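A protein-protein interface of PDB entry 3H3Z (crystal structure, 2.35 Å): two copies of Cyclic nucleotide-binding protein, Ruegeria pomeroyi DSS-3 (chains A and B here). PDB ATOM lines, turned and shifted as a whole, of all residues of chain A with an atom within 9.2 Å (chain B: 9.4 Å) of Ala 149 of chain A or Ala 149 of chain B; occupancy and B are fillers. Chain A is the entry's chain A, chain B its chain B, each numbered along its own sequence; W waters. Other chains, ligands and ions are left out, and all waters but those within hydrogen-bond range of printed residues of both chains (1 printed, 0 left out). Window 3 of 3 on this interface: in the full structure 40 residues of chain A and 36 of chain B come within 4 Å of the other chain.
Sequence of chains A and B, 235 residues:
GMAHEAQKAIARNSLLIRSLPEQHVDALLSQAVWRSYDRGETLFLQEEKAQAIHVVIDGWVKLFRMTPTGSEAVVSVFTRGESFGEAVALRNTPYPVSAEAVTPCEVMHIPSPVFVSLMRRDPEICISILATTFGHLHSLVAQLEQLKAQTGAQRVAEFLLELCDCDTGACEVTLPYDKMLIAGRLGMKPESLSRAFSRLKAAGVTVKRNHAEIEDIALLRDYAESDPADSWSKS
The backbone carbonyl oxygen (O) of Glu 145 of chain A sits at hydrogen-bond distance from the guanidinium group (NH1) of Arg 155 of chain B, 3.2 Å away. The backbone carbonyl oxygen (O) of Gln 146 of chain A sits close to the guanidinium group (NH1) of Arg 155 of chain B, at 3.4 Å. O of Leu 147 of chain A is in hydrogen-bond range of NE of Arg 155 of chain B, 3.2 Å away. The backbone carbonyl oxygen (O) of Lys 148 of chain B sits at hydrogen-bond distance from the backbone NH (N) of Gln 150 of chain A, 3.4 Å away. O of Leu 186 of chain A sits at hydrogen-bond distance from N of Leu 147 of chain B (2.9 Å).
The guanidinium group of Arg 155 of chain A sits at hydrogen-bond distance from the side-chain amide oxygen of Gln 150 of chain A (3.0 Å). The backbone NH (N) of Thr 151 of chain A sits at hydrogen-bond distance from the side-chain amide oxygen (OE1) of Gln 154 of chain A, 2.9 Å away. The side-chain amino group (NZ) of Lys 148 of chain B is in salt-bridge range of the side-chain carboxylate (OE1) of Glu 158 of chain B, 3.6 Å away. OE1 of Glu 158 of chain B sits close to OE1 of Gln 150 of chain B (2.7 Å). The side-chain amide nitrogen (NE2) of Gln 150 of chain B lies within hydrogen-bond range of the backbone carbonyl oxygen (O) of Ala 224 of chain B, 3.0 Å away. The guanidinium group (NH1) of Arg 155 of chain B is in hydrogen-bond range of the backbone carbonyl oxygen (O) of Leu 186 of chain B, 2.5 Å away.
Among the printed residues, merely in contact across the chains: Glu 145 of chain A with Leu 186 of chain B, Gln 146 of chain A with Leu 186 of chain B, Gln 146 of chain A with Gly 187 of chain B, Leu 147 of chain A with Lys 148 of chain B, Lys 148 of chain A with Arg 155 of chain B, Ala 149 of chain A with Lys 148 of chain B, Ala 149 of chain A with Ala 149 of chain B, Ala 149 of chain A with Gln 150 of chain B, Gln 150 of chain A with Leu 147 of chain B, Thr 151 of chain A with Leu 147 of chain B, Gly 152 of chain A with Leu 147 of chain B, Arg 155 of chain A with Leu 147 of chain B, Leu 186 of chain A with Gln 146 of chain B, Gly 187 of chain A with Gln 146 of chain B and Met 188 of chain A with Leu 147 of chain B.
Lys 148 of chain A touches one residue of chain B. Ala 149 of chain A touches just these residues of chain B: Lys 148 (3.4 Å), Ala 149 (3.5 Å) and Gln 150 (3.1 Å). Of the printed residues of chain B, Gln 150 of chain A touches Leu 147 (3.5 Å) and Lys 148 (3.4 Å). Of the printed residues of chain B, Arg 155 of chain A touches Leu 147 (3.2 Å). Of the printed residues of chain B, Met 188 of chain A touches Leu 147 (3.8 Å). Ala 149 of chain B touches one residue of chain A. Of the printed residues of chain A, Gln 150 of chain B touches Ala 149. Glu 225 of chain B touches none of the printed residues of chain A. The nearest residue of chain B that does not touch Ala 149 of chain A is Thr 151 of chain B (5.0 Å).
Along chain A the printed residues that touch a printed residue of chain B span positions 145 to 188. Printed residues of chain B that touch a printed residue of chain A: Gln 146, Leu 147, Lys 148, Ala 149, Gln 150, Arg 155, Leu 186 and Gly 187.
Gln 146 of chain A touches Leu 186 of chain B, and with the chains exchanged Leu 186 of chain A touches Gln 146 of chain B. Gln 146 of chain A touches Gly 187 of chain B, and with the chains exchanged Gly 187 of chain A touches Gln 146 of chain B. Leu 147 of chain A touches Lys 148 of chain B, but with the chains exchanged Lys 148 of chain A does not touch Leu 147 of chain B (6.8 Å). Ala 149 of chain A touches Lys 148 of chain B, but with the chains exchanged Lys 148 of chain A does not touch Ala 149 of chain B (6.1 Å). Of the 20 pairs that touch across the chains among the printed residues, 7 have their exchanged pair printed and touching as well.
Water W1 bridges O of Gln 150 of chain B (2.8 Å) and N of Ala 149 of chain A (3.2 Å).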
ATOM      1  N   LEU A 144      -8.334  -1.380 -13.939  1.00  0.00           N
ATOM      2  CA  LEU A 144      -8.314  -0.208 -13.066  1.00  0.00           C
ATOM      3  C   LEU A 144      -6.978  -0.100 -12.421  1.00  0.00           C
ATOM      4  O   LEU A 144      -6.455   0.958 -12.305  1.00  0.00           O
ATOM      5  CB  LEU A 144      -9.413  -0.221 -11.978  1.00  0.00           C
ATOM      6  CG  LEU A 144     -10.786   0.335 -12.382  1.00  0.00           C
ATOM      7  CD1 LEU A 144     -11.829   0.110 -11.292  1.00  0.00           C
ATOM      8  CD2 LEU A 144     -10.690   1.818 -12.678  1.00  0.00           C
ATOM      9  N   GLU A 145      -6.410  -1.205 -12.002  1.00  0.00           N
ATOM     10  CA  GLU A 145      -5.091  -1.144 -11.391  1.00  0.00           C
ATOM     11  C   GLU A 145      -3.968  -0.689 -12.332  1.00  0.00           C
ATOM     12  O   GLU A 145      -2.942  -0.274 -11.865  1.00  0.00           O
ATOM     13  CB  GLU A 145      -4.702  -2.496 -10.860  1.00  0.00           C
ATOM     14  CG  GLU A 145      -5.618  -2.997  -9.839  1.00  0.00           C
ATOM     15  CD  GLU A 145      -4.966  -4.053  -9.041  1.00  0.00           C
ATOM     16  OE1 GLU A 145      -4.226  -3.656  -8.091  1.00  0.00           O
ATOM     17  OE2 GLU A 145      -5.187  -5.237  -9.386  1.00  0.00           O
ATOM     18  N   GLN A 146      -4.185  -0.798 -13.629  1.00  0.00           N
ATOM     19  CA  GLN A 146      -3.214  -0.468 -14.659  1.00  0.00           C
ATOM     20  C   GLN A 146      -3.516   0.791 -15.399  1.00  0.00           C
ATOM     21  O   GLN A 146      -2.762   1.190 -16.269  1.00  0.00           O
ATOM     22  CB  GLN A 146      -3.203  -1.603 -15.683  1.00  0.00           C
ATOM     23  CG  GLN A 146      -2.648  -2.842 -15.086  1.00  0.00           C
ATOM     24  CD  GLN A 146      -2.739  -3.992 -15.999  1.00  0.00           C
ATOM     25  OE1 GLN A 146      -3.034  -3.837 -17.176  1.00  0.00           O
ATOM     26  NE2 GLN A 146      -2.537  -5.174 -15.459  1.00  0.00           N
ATOM     27  N   LEU A 147      -4.641   1.405 -15.071  1.00  0.00           N
ATOM     28  CA  LEU A 147      -5.066   2.581 -15.747  1.00  0.00           C
ATOM     29  C   LEU A 147      -4.034   3.684 -15.455  1.00  0.00           C
ATOM     30  O   LEU A 147      -3.815   4.035 -14.281  1.00  0.00           O
ATOM     31  CB  LEU A 147      -6.456   2.956 -15.255  1.00  0.00           C
ATOM     32  CG  LEU A 147      -7.120   4.111 -15.993  1.00  0.00           C
ATOM     33  CD1 LEU A 147      -7.521   3.674 -17.416  1.00  0.00           C
ATOM     34  CD2 LEU A 147      -8.318   4.646 -15.192  1.00  0.00           C
ATOM     35  N   LYS A 148      -3.373   4.171 -16.515  1.00  0.00           N
ATOM     36  CA  LYS A 148      -2.411   5.257 -16.407  1.00  0.00           C
ATOM     37  C   LYS A 148      -3.163   6.581 -16.631  1.00  0.00           C
ATOM     38  O   LYS A 148      -4.273   6.575 -17.175  1.00  0.00           O
ATOM     39  CB  LYS A 148      -1.267   5.115 -17.438  1.00  0.00           C
ATOM     40  CG  LYS A 148      -0.332   3.881 -17.291  1.00  0.00           C
ATOM     41  N   ALA A 149      -2.578   7.701 -16.188  1.00  0.00           N
ATOM     42  CA  ALA A 149      -3.138   9.033 -16.462  1.00  0.00           C
ATOM     43  C   ALA A 149      -3.050   9.315 -17.952  1.00  0.00           C
ATOM     44  O   ALA A 149      -2.228   8.729 -18.654  1.00  0.00           O
ATOM     45  CB  ALA A 149      -2.428  10.150 -15.662  1.00  0.00           C
ATOM     46  N   GLN A 150      -3.958  10.166 -18.419  1.00  0.00           N
ATOM     47  CA  GLN A 150      -4.000  10.618 -19.806  1.00  0.00           C
ATOM     48  C   GLN A 150      -4.637  11.996 -19.800  1.00  0.00           C
ATOM     49  O   GLN A 150      -5.173  12.427 -18.765  1.00  0.00           O
ATOM     50  CB  GLN A 150      -4.809   9.684 -20.691  1.00  0.00           C
ATOM     51  CG  GLN A 150      -6.347   9.784 -20.449  1.00  0.00           C
ATOM     52  CD  GLN A 150      -7.156   8.852 -21.325  1.00  0.00           C
ATOM     53  OE1 GLN A 150      -8.339   8.641 -21.081  1.00  0.00           O
ATOM     54  NE2 GLN A 150      -6.526   8.299 -22.360  1.00  0.00           N
ATOM     55  N   THR A 151      -4.640  12.666 -20.947  1.00  0.00           N
ATOM     56  CA  THR A 151      -5.233  14.013 -21.011  1.00  0.00           C
ATOM     57  C   THR A 151      -6.734  13.912 -21.251  1.00  0.00           C
ATOM     58  O   THR A 151      -7.213  12.927 -21.802  1.00  0.00           O
ATOM     59  CB  THR A 151      -4.611  14.863 -22.128  1.00  0.00           C
ATOM     60  OG1 THR A 151      -5.024  14.346 -23.385  1.00  0.00           O
ATOM     61  CG2 THR A 151      -3.064  14.837 -22.060  1.00  0.00           C
ATOM     62  N   GLY A 152      -7.463  14.942 -20.842  1.00  0.00           N
ATOM     63  CA  GLY A 152      -8.902  15.015 -21.060  1.00  0.00           C
ATOM     64  C   GLY A 152      -9.309  14.859 -22.516  1.00  0.00           C
ATOM     65  O   GLY A 152     -10.354  14.274 -22.815  1.00  0.00           O
ATOM     66  N   GLN A 154      -7.559  13.177 -24.746  1.00  0.00           N
ATOM     67  CA  GLN A 154      -7.334  11.764 -25.028  1.00  0.00           C
ATOM     68  C   GLN A 154      -8.548  10.900 -24.551  1.00  0.00           C
ATOM     69  O   GLN A 154      -8.928   9.978 -25.259  1.00  0.00           O
ATOM     70  CB  GLN A 154      -6.006  11.293 -24.404  1.00  0.00           C
ATOM     71  CG  GLN A 154      -4.759  11.731 -25.176  1.00  0.00           C
ATOM     72  CD  GLN A 154      -3.471  11.322 -24.463  1.00  0.00           C
ATOM     73  OE1 GLN A 154      -3.217  11.719 -23.309  1.00  0.00           O
ATOM     74  NE2 GLN A 154      -2.643  10.535 -25.159  1.00  0.00           N
ATOM     75  N   ARG A 155      -9.094  11.201 -23.351  1.00  0.00           N
ATOM     76  CA  ARG A 155     -10.348  10.607 -22.833  1.00  0.00           C
ATOM     77  C   ARG A 155     -11.468  10.798 -23.831  1.00  0.00           C
ATOM     78  O   ARG A 155     -12.170   9.854 -24.160  1.00  0.00           O
ATOM     79  CB  ARG A 155     -10.849  11.271 -21.537  1.00  0.00           C
ATOM     80  CG  ARG A 155     -10.691  10.554 -20.186  1.00  0.00           C
ATOM     81  CD  ARG A 155     -11.665   9.382 -19.993  1.00  0.00           C
ATOM     82  NE  ARG A 155     -11.290   8.232 -20.819  1.00  0.00           N
ATOM     83  CZ  ARG A 155     -12.138   7.366 -21.378  1.00  0.00           C
ATOM     84  NH1 ARG A 155     -13.454   7.452 -21.211  1.00  0.00           N
ATOM     85  NH2 ARG A 155     -11.648   6.396 -22.146  1.00  0.00           N
ATOM     86  N   GLU A 158     -10.903   8.809 -27.186  1.00  0.00           N
ATOM     87  CA  GLU A 158     -11.200   7.413 -26.900  1.00  0.00           C
ATOM     88  C   GLU A 158     -12.684   7.133 -26.802  1.00  0.00           C
ATOM     89  O   GLU A 158     -13.196   6.144 -27.362  1.00  0.00           O
ATOM     90  CB  GLU A 158     -10.526   7.021 -25.589  1.00  0.00           C
ATOM     91  CG  GLU A 158      -9.067   6.692 -25.778  1.00  0.00           C
ATOM     92  CD  GLU A 158      -8.381   6.315 -24.503  1.00  0.00           C
ATOM     93  OE1 GLU A 158      -8.872   6.705 -23.417  1.00  0.00           O
ATOM     94  OE2 GLU A 158      -7.331   5.642 -24.589  1.00  0.00           O
ATOM     95  N   LEU A 186     -17.618  11.053 -18.309  1.00  0.00           N
ATOM     96  CA  LEU A 186     -16.152  11.018 -18.397  1.00  0.00           C
ATOM     97  C   LEU A 186     -15.423  11.527 -17.137  1.00  0.00           C
ATOM     98  O   LEU A 186     -14.180  11.547 -17.127  1.00  0.00           O
ATOM     99  CB  LEU A 186     -15.661  11.795 -19.624  1.00  0.00           C
ATOM    100  CG  LEU A 186     -16.221  11.267 -20.953  1.00  0.00           C
ATOM    101  CD1 LEU A 186     -15.601  12.020 -22.097  1.00  0.00           C
ATOM    102  CD2 LEU A 186     -16.006   9.761 -21.143  1.00  0.00           C
ATOM    103  N   GLY A 187     -16.179  11.898 -16.091  1.00  0.00           N
ATOM    104  CA  GLY A 187     -15.626  12.423 -14.855  1.00  0.00           C
ATOM    105  C   GLY A 187     -14.816  13.710 -15.043  1.00  0.00           C
ATOM    106  O   GLY A 187     -13.792  13.922 -14.384  1.00  0.00           O
ATOM    107  N   MET A 188     -15.288  14.577 -15.924  1.00  0.00           N
ATOM    108  CA  MET A 188     -14.606  15.817 -16.243  1.00  0.00           C
ATOM    109  C   MET A 188     -15.418  17.044 -15.888  1.00  0.00           C
ATOM    110  O   MET A 188     -16.645  16.987 -15.699  1.00  0.00           O
ATOM    111  CB  MET A 188     -14.284  15.850 -17.727  1.00  0.00           C
ATOM    112  CG  MET A 188     -13.259  14.797 -18.096  1.00  0.00           C
ATOM    113  SD  MET A 188     -13.056  14.677 -20.000  1.00  0.00           S
ATOM    114  CE  MET A 188     -12.380  16.562 -20.364  1.00  0.00           C
ATOM    115  N   ALA A 224      -5.177   9.790 -29.704  1.00  0.00           N
ATOM    116  CA  ALA A 224      -5.516   9.181 -28.423  1.00  0.00           C
ATOM    117  C   ALA A 224      -4.374   8.337 -27.914  1.00  0.00           C
ATOM    118  O   ALA A 224      -4.178   8.237 -26.696  1.00  0.00           O
ATOM    119  CB  ALA A 224      -6.784   8.345 -28.553  1.00  0.00           C
ATOM    120  N   SER A 226      -1.068   8.863 -28.022  1.00  0.00           N
ATOM    121  CA  SER A 226       0.104   9.748 -28.083  1.00  0.00           C
ATOM    122  C   SER A 226       0.577  10.190 -26.691  1.00  0.00           C
ATOM    123  O   SER A 226       0.067   9.702 -25.683  1.00  0.00           O
ATOM    124  CB  SER A 226      -0.237  10.975 -28.929  1.00  0.00           C
ATOM    125  N   ASP A 227       1.554  11.103 -26.642  1.00  0.00           N
ATOM    126  CA  ASP A 227       2.103  11.638 -25.375  1.00  0.00           C
ATOM    127  C   ASP A 227       1.130  12.589 -24.691  1.00  0.00           C
ATOM    128  O   ASP A 227       1.310  12.940 -23.522  1.00  0.00           O
ATOM    129  CB  ASP A 227       3.431  12.373 -25.614  1.00  0.00           C
ATOM    130  N   GLN B 146     -14.067   7.241 -16.324  1.00  0.00           N
ATOM    131  CA  GLN B 146     -13.733   8.505 -15.710  1.00  0.00           C
ATOM    132  C   GLN B 146     -12.231   8.791 -15.759  1.00  0.00           C
ATOM    133  O   GLN B 146     -11.399   7.941 -15.405  1.00  0.00           O
ATOM    134  CB  GLN B 146     -14.277   8.522 -14.287  1.00  0.00           C
ATOM    135  CG  GLN B 146     -15.798   8.528 -14.328  1.00  0.00           C
ATOM    136  CD  GLN B 146     -16.405   8.280 -13.010  1.00  0.00           C
ATOM    137  OE1 GLN B 146     -15.714   8.242 -11.986  1.00  0.00           O
ATOM    138  NE2 GLN B 146     -17.718   8.078 -13.005  1.00  0.00           N
ATOM    139  N   LEU B 147     -11.923   9.997 -16.226  1.00  0.00           N
ATOM    140  CA  LEU B 147     -10.557  10.496 -16.418  1.00  0.00           C
ATOM    141  C   LEU B 147      -9.629  10.246 -15.231  1.00  0.00           C
ATOM    142  O   LEU B 147      -9.955  10.641 -14.114  1.00  0.00           O
ATOM    143  CB  LEU B 147     -10.603  12.010 -16.700  1.00  0.00           C
ATOM    144  CG  LEU B 147      -9.309  12.762 -17.098  1.00  0.00           C
ATOM    145  CD1 LEU B 147      -8.649  12.162 -18.350  1.00  0.00           C
ATOM    146  CD2 LEU B 147      -9.600  14.267 -17.279  1.00  0.00           C
ATOM    147  N   LYS B 148      -8.511   9.547 -15.461  1.00  0.00           N
ATOM    148  CA  LYS B 148      -7.510   9.381 -14.411  1.00  0.00           C
ATOM    149  C   LYS B 148      -6.469  10.454 -14.651  1.00  0.00           C
ATOM    150  O   LYS B 148      -6.062  10.670 -15.783  1.00  0.00           O
ATOM    151  CB  LYS B 148      -6.865   7.984 -14.392  1.00  0.00           C
ATOM    152  CG  LYS B 148      -6.135   7.720 -13.053  1.00  0.00           C
ATOM    153  CD  LYS B 148      -6.133   6.260 -12.546  1.00  0.00           C
ATOM    154  CE  LYS B 148      -5.672   6.269 -11.076  1.00  0.00           C
ATOM    155  NZ  LYS B 148      -5.659   4.994 -10.309  1.00  0.00           N
ATOM    156  N   ALA B 149      -6.088  11.145 -13.594  1.00  0.00           N
ATOM    157  CA  ALA B 149      -5.107  12.230 -13.653  1.00  0.00           C
ATOM    158  C   ALA B 149      -3.825  11.932 -12.865  1.00  0.00           C
ATOM    159  O   ALA B 149      -2.773  12.516 -13.141  1.00  0.00           O
ATOM    160  CB  ALA B 149      -5.750  13.549 -13.146  1.00  0.00           C
ATOM    161  N   GLN B 150      -3.915  11.027 -11.896  1.00  0.00           N
ATOM    162  CA  GLN B 150      -2.784  10.646 -11.050  1.00  0.00           C
ATOM    163  C   GLN B 150      -1.494  10.163 -11.727  1.00  0.00           C
ATOM    164  O   GLN B 150      -1.500   9.482 -12.764  1.00  0.00           O
ATOM    165  CB  GLN B 150      -3.224   9.566 -10.087  1.00  0.00           C
ATOM    166  CG  GLN B 150      -4.019  10.127  -8.952  1.00  0.00           C
ATOM    167  CD  GLN B 150      -4.481   9.047  -8.043  1.00  0.00           C
ATOM    168  OE1 GLN B 150      -4.784   7.931  -8.495  1.00  0.00           O
ATOM    169  NE2 GLN B 150      -4.546   9.352  -6.742  1.00  0.00           N
ATOM    170  N   THR B 151      -0.391  10.530 -11.076  1.00  0.00           N
ATOM    171  CA  THR B 151       0.940  10.207 -11.535  1.00  0.00           C
ATOM    172  C   THR B 151       1.293   8.817 -11.028  1.00  0.00           C
ATOM    173  O   THR B 151       0.636   8.310 -10.086  1.00  0.00           O
ATOM    174  CB  THR B 151       1.970  11.243 -11.008  1.00  0.00           C
ATOM    175  OG1 THR B 151       1.988  11.216  -9.580  1.00  0.00           O
ATOM    176  CG2 THR B 151       1.627  12.662 -11.464  1.00  0.00           C
ATOM    177  N   GLY B 152       2.320   8.215 -11.636  1.00  0.00           N
ATOM    178  CA  GLY B 152       2.835   6.913 -11.197  1.00  0.00           C
ATOM    179  C   GLY B 152       3.042   6.810  -9.688  1.00  0.00           C
ATOM    180  O   GLY B 152       2.615   5.838  -9.043  1.00  0.00           O
ATOM    181  N   ALA B 153       3.664   7.830  -9.104  1.00  0.00           N
ATOM    182  CA  ALA B 153       3.973   7.796  -7.689  1.00  0.00           C
ATOM    183  C   ALA B 153       2.703   7.871  -6.862  1.00  0.00           C
ATOM    184  O   ALA B 153       2.630   7.340  -5.725  1.00  0.00           O
ATOM    185  CB  ALA B 153       4.947   8.943  -7.331  1.00  0.00           C
ATOM    186  N   GLN B 154       1.695   8.542  -7.422  1.00  0.00           N
ATOM    187  CA  GLN B 154       0.409   8.634  -6.732  1.00  0.00           C
ATOM    188  C   GLN B 154      -0.267   7.272  -6.743  1.00  0.00           C
ATOM    189  O   GLN B 154      -0.746   6.790  -5.699  1.00  0.00           O
ATOM    190  CB  GLN B 154      -0.454   9.709  -7.366  1.00  0.00           C
ATOM    191  CG  GLN B 154       0.043  11.087  -7.050  1.00  0.00           C
ATOM    192  CD  GLN B 154      -0.739  12.152  -7.749  1.00  0.00           C
ATOM    193  OE1 GLN B 154      -0.829  12.198  -8.994  1.00  0.00           O
ATOM    194  NE2 GLN B 154      -1.298  13.036  -6.963  1.00  0.00           N
ATOM    195  N   ARG B 155      -0.238   6.625  -7.909  1.00  0.00           N
ATOM    196  CA  ARG B 155      -0.796   5.277  -8.056  1.00  0.00           C
ATOM    197  C   ARG B 155      -0.096   4.324  -7.106  1.00  0.00           C
ATOM    198  O   ARG B 155      -0.763   3.582  -6.371  1.00  0.00           O
ATOM    199  CB  ARG B 155      -0.689   4.801  -9.493  1.00  0.00           C
ATOM    200  CG  ARG B 155      -1.559   5.617 -10.445  1.00  0.00           C
ATOM    201  CD  ARG B 155      -1.184   5.316 -11.863  1.00  0.00           C
ATOM    202  NE  ARG B 155      -1.426   3.914 -12.183  1.00  0.00           N
ATOM    203  CZ  ARG B 155      -0.840   3.235 -13.165  1.00  0.00           C
ATOM    204  NH1 ARG B 155      -1.175   1.972 -13.354  1.00  0.00           N
ATOM    205  NH2 ARG B 155       0.072   3.790 -13.949  1.00  0.00           N
ATOM    206  N   GLU B 158      -1.334   5.014  -3.660  1.00  0.00           N
ATOM    207  CA  GLU B 158      -2.652   4.423  -3.472  1.00  0.00           C
ATOM    208  C   GLU B 158      -2.615   2.930  -3.328  1.00  0.00           C
ATOM    209  O   GLU B 158      -3.414   2.351  -2.586  1.00  0.00           O
ATOM    210  CB  GLU B 158      -3.521   4.709  -4.674  1.00  0.00           C
ATOM    211  CG  GLU B 158      -3.956   6.087  -4.708  1.00  0.00           C
ATOM    212  CD  GLU B 158      -4.701   6.406  -5.948  1.00  0.00           C
ATOM    213  OE1 GLU B 158      -4.474   5.738  -7.002  1.00  0.00           O
ATOM    214  OE2 GLU B 158      -5.511   7.353  -5.848  1.00  0.00           O
ATOM    215  N   LEU B 186       0.661  -3.007 -11.466  1.00  0.00           N
ATOM    216  CA  LEU B 186       0.314  -1.610 -11.654  1.00  0.00           C
ATOM    217  C   LEU B 186       0.475  -1.181 -13.102  1.00  0.00           C
ATOM    218  O   LEU B 186       0.358  -0.007 -13.389  1.00  0.00           O
ATOM    219  CB  LEU B 186       1.150  -0.713 -10.720  1.00  0.00           C
ATOM    220  CG  LEU B 186       0.981  -1.057  -9.217  1.00  0.00           C
ATOM    221  CD1 LEU B 186       1.844  -0.211  -8.278  1.00  0.00           C
ATOM    222  CD2 LEU B 186      -0.495  -0.939  -8.811  1.00  0.00           C
ATOM    223  N   GLY B 187       0.737  -2.110 -14.022  1.00  0.00           N
ATOM    224  CA  GLY B 187       0.915  -1.725 -15.434  1.00  0.00           C
ATOM    225  C   GLY B 187       2.046  -0.704 -15.656  1.00  0.00           C
ATOM    226  O   GLY B 187       1.949   0.164 -16.526  1.00  0.00           O
ATOM    227  N   MET B 188       3.107  -0.819 -14.864  1.00  0.00           N
ATOM    228  CA  MET B 188       4.229   0.109 -14.892  1.00  0.00           C
ATOM    229  C   MET B 188       5.540  -0.535 -15.319  1.00  0.00           C
ATOM    230  O   MET B 188       5.842  -1.681 -14.941  1.00  0.00           O
ATOM    231  CB  MET B 188       4.458   0.694 -13.505  1.00  0.00           C
ATOM    232  CG  MET B 188       3.418   1.699 -13.083  1.00  0.00           C
ATOM    233  SD  MET B 188       3.885   2.359 -11.368  1.00  0.00           S
ATOM    234  CE  MET B 188       5.356   3.423 -11.860  1.00  0.00           C
ATOM    235  N   ALA B 224      -1.080  11.389  -2.505  1.00  0.00           N
ATOM    236  CA  ALA B 224      -1.961  10.698  -3.433  1.00  0.00           C
ATOM    237  C   ALA B 224      -3.095  11.595  -3.914  1.00  0.00           C
ATOM    238  O   ALA B 224      -3.392  11.627  -5.106  1.00  0.00           O
ATOM    239  CB  ALA B 224      -2.518   9.428  -2.779  1.00  0.00           C
ATOM    240  N   GLU B 225      -3.711  12.331  -2.987  1.00  0.00           N
ATOM    241  CA  GLU B 225      -4.861  13.210  -3.301  1.00  0.00           C
ATOM    242  C   GLU B 225      -4.486  14.557  -3.934  1.00  0.00           C
ATOM    243  O   GLU B 225      -5.313  15.133  -4.639  1.00  0.00           O
ATOM    244  CB  GLU B 225      -5.701  13.433  -2.054  1.00  0.00           C
ATOM    245  CG  GLU B 225      -6.436  12.173  -1.617  1.00  0.00           C
ATOM    246  CD  GLU B 225      -7.073  12.299  -0.228  1.00  0.00           C
ATOM    247  OE1 GLU B 225      -6.676  13.209   0.554  1.00  0.00           O
ATOM    248  OE2 GLU B 225      -7.968  11.475   0.087  1.00  0.00           O
ATOM    249  N   SER B 226      -3.258  15.035  -3.693  1.00  0.00           N
ATOM    250  CA  SER B 226      -2.718  16.265  -4.294  1.00  0.00           C
ATOM    251  C   SER B 226      -2.970  16.393  -5.808  1.00  0.00           C
ATOM    252  O   SER B 226      -3.091  15.389  -6.500  1.00  0.00           O
ATOM    253  CB  SER B 226      -1.206  16.332  -4.036  1.00  0.00           C
ATOM    254  N   ASP B 227      -3.044  17.631  -6.310  1.00  0.00           N
ATOM    255  CA  ASP B 227      -3.262  17.911  -7.739  1.00  0.00           C
ATOM    256  C   ASP B 227      -1.942  18.225  -8.446  1.00  0.00           C
ATOM    257  O   ASP B 227      -1.576  17.564  -9.429  1.00  0.00           O
ATOM    258  CB  ASP B 227      -4.246  19.074  -7.938  1.00  0.00           C
HETATM  259  O   HOH W   1      -0.235   7.380 -14.042  1.00  0.00           O
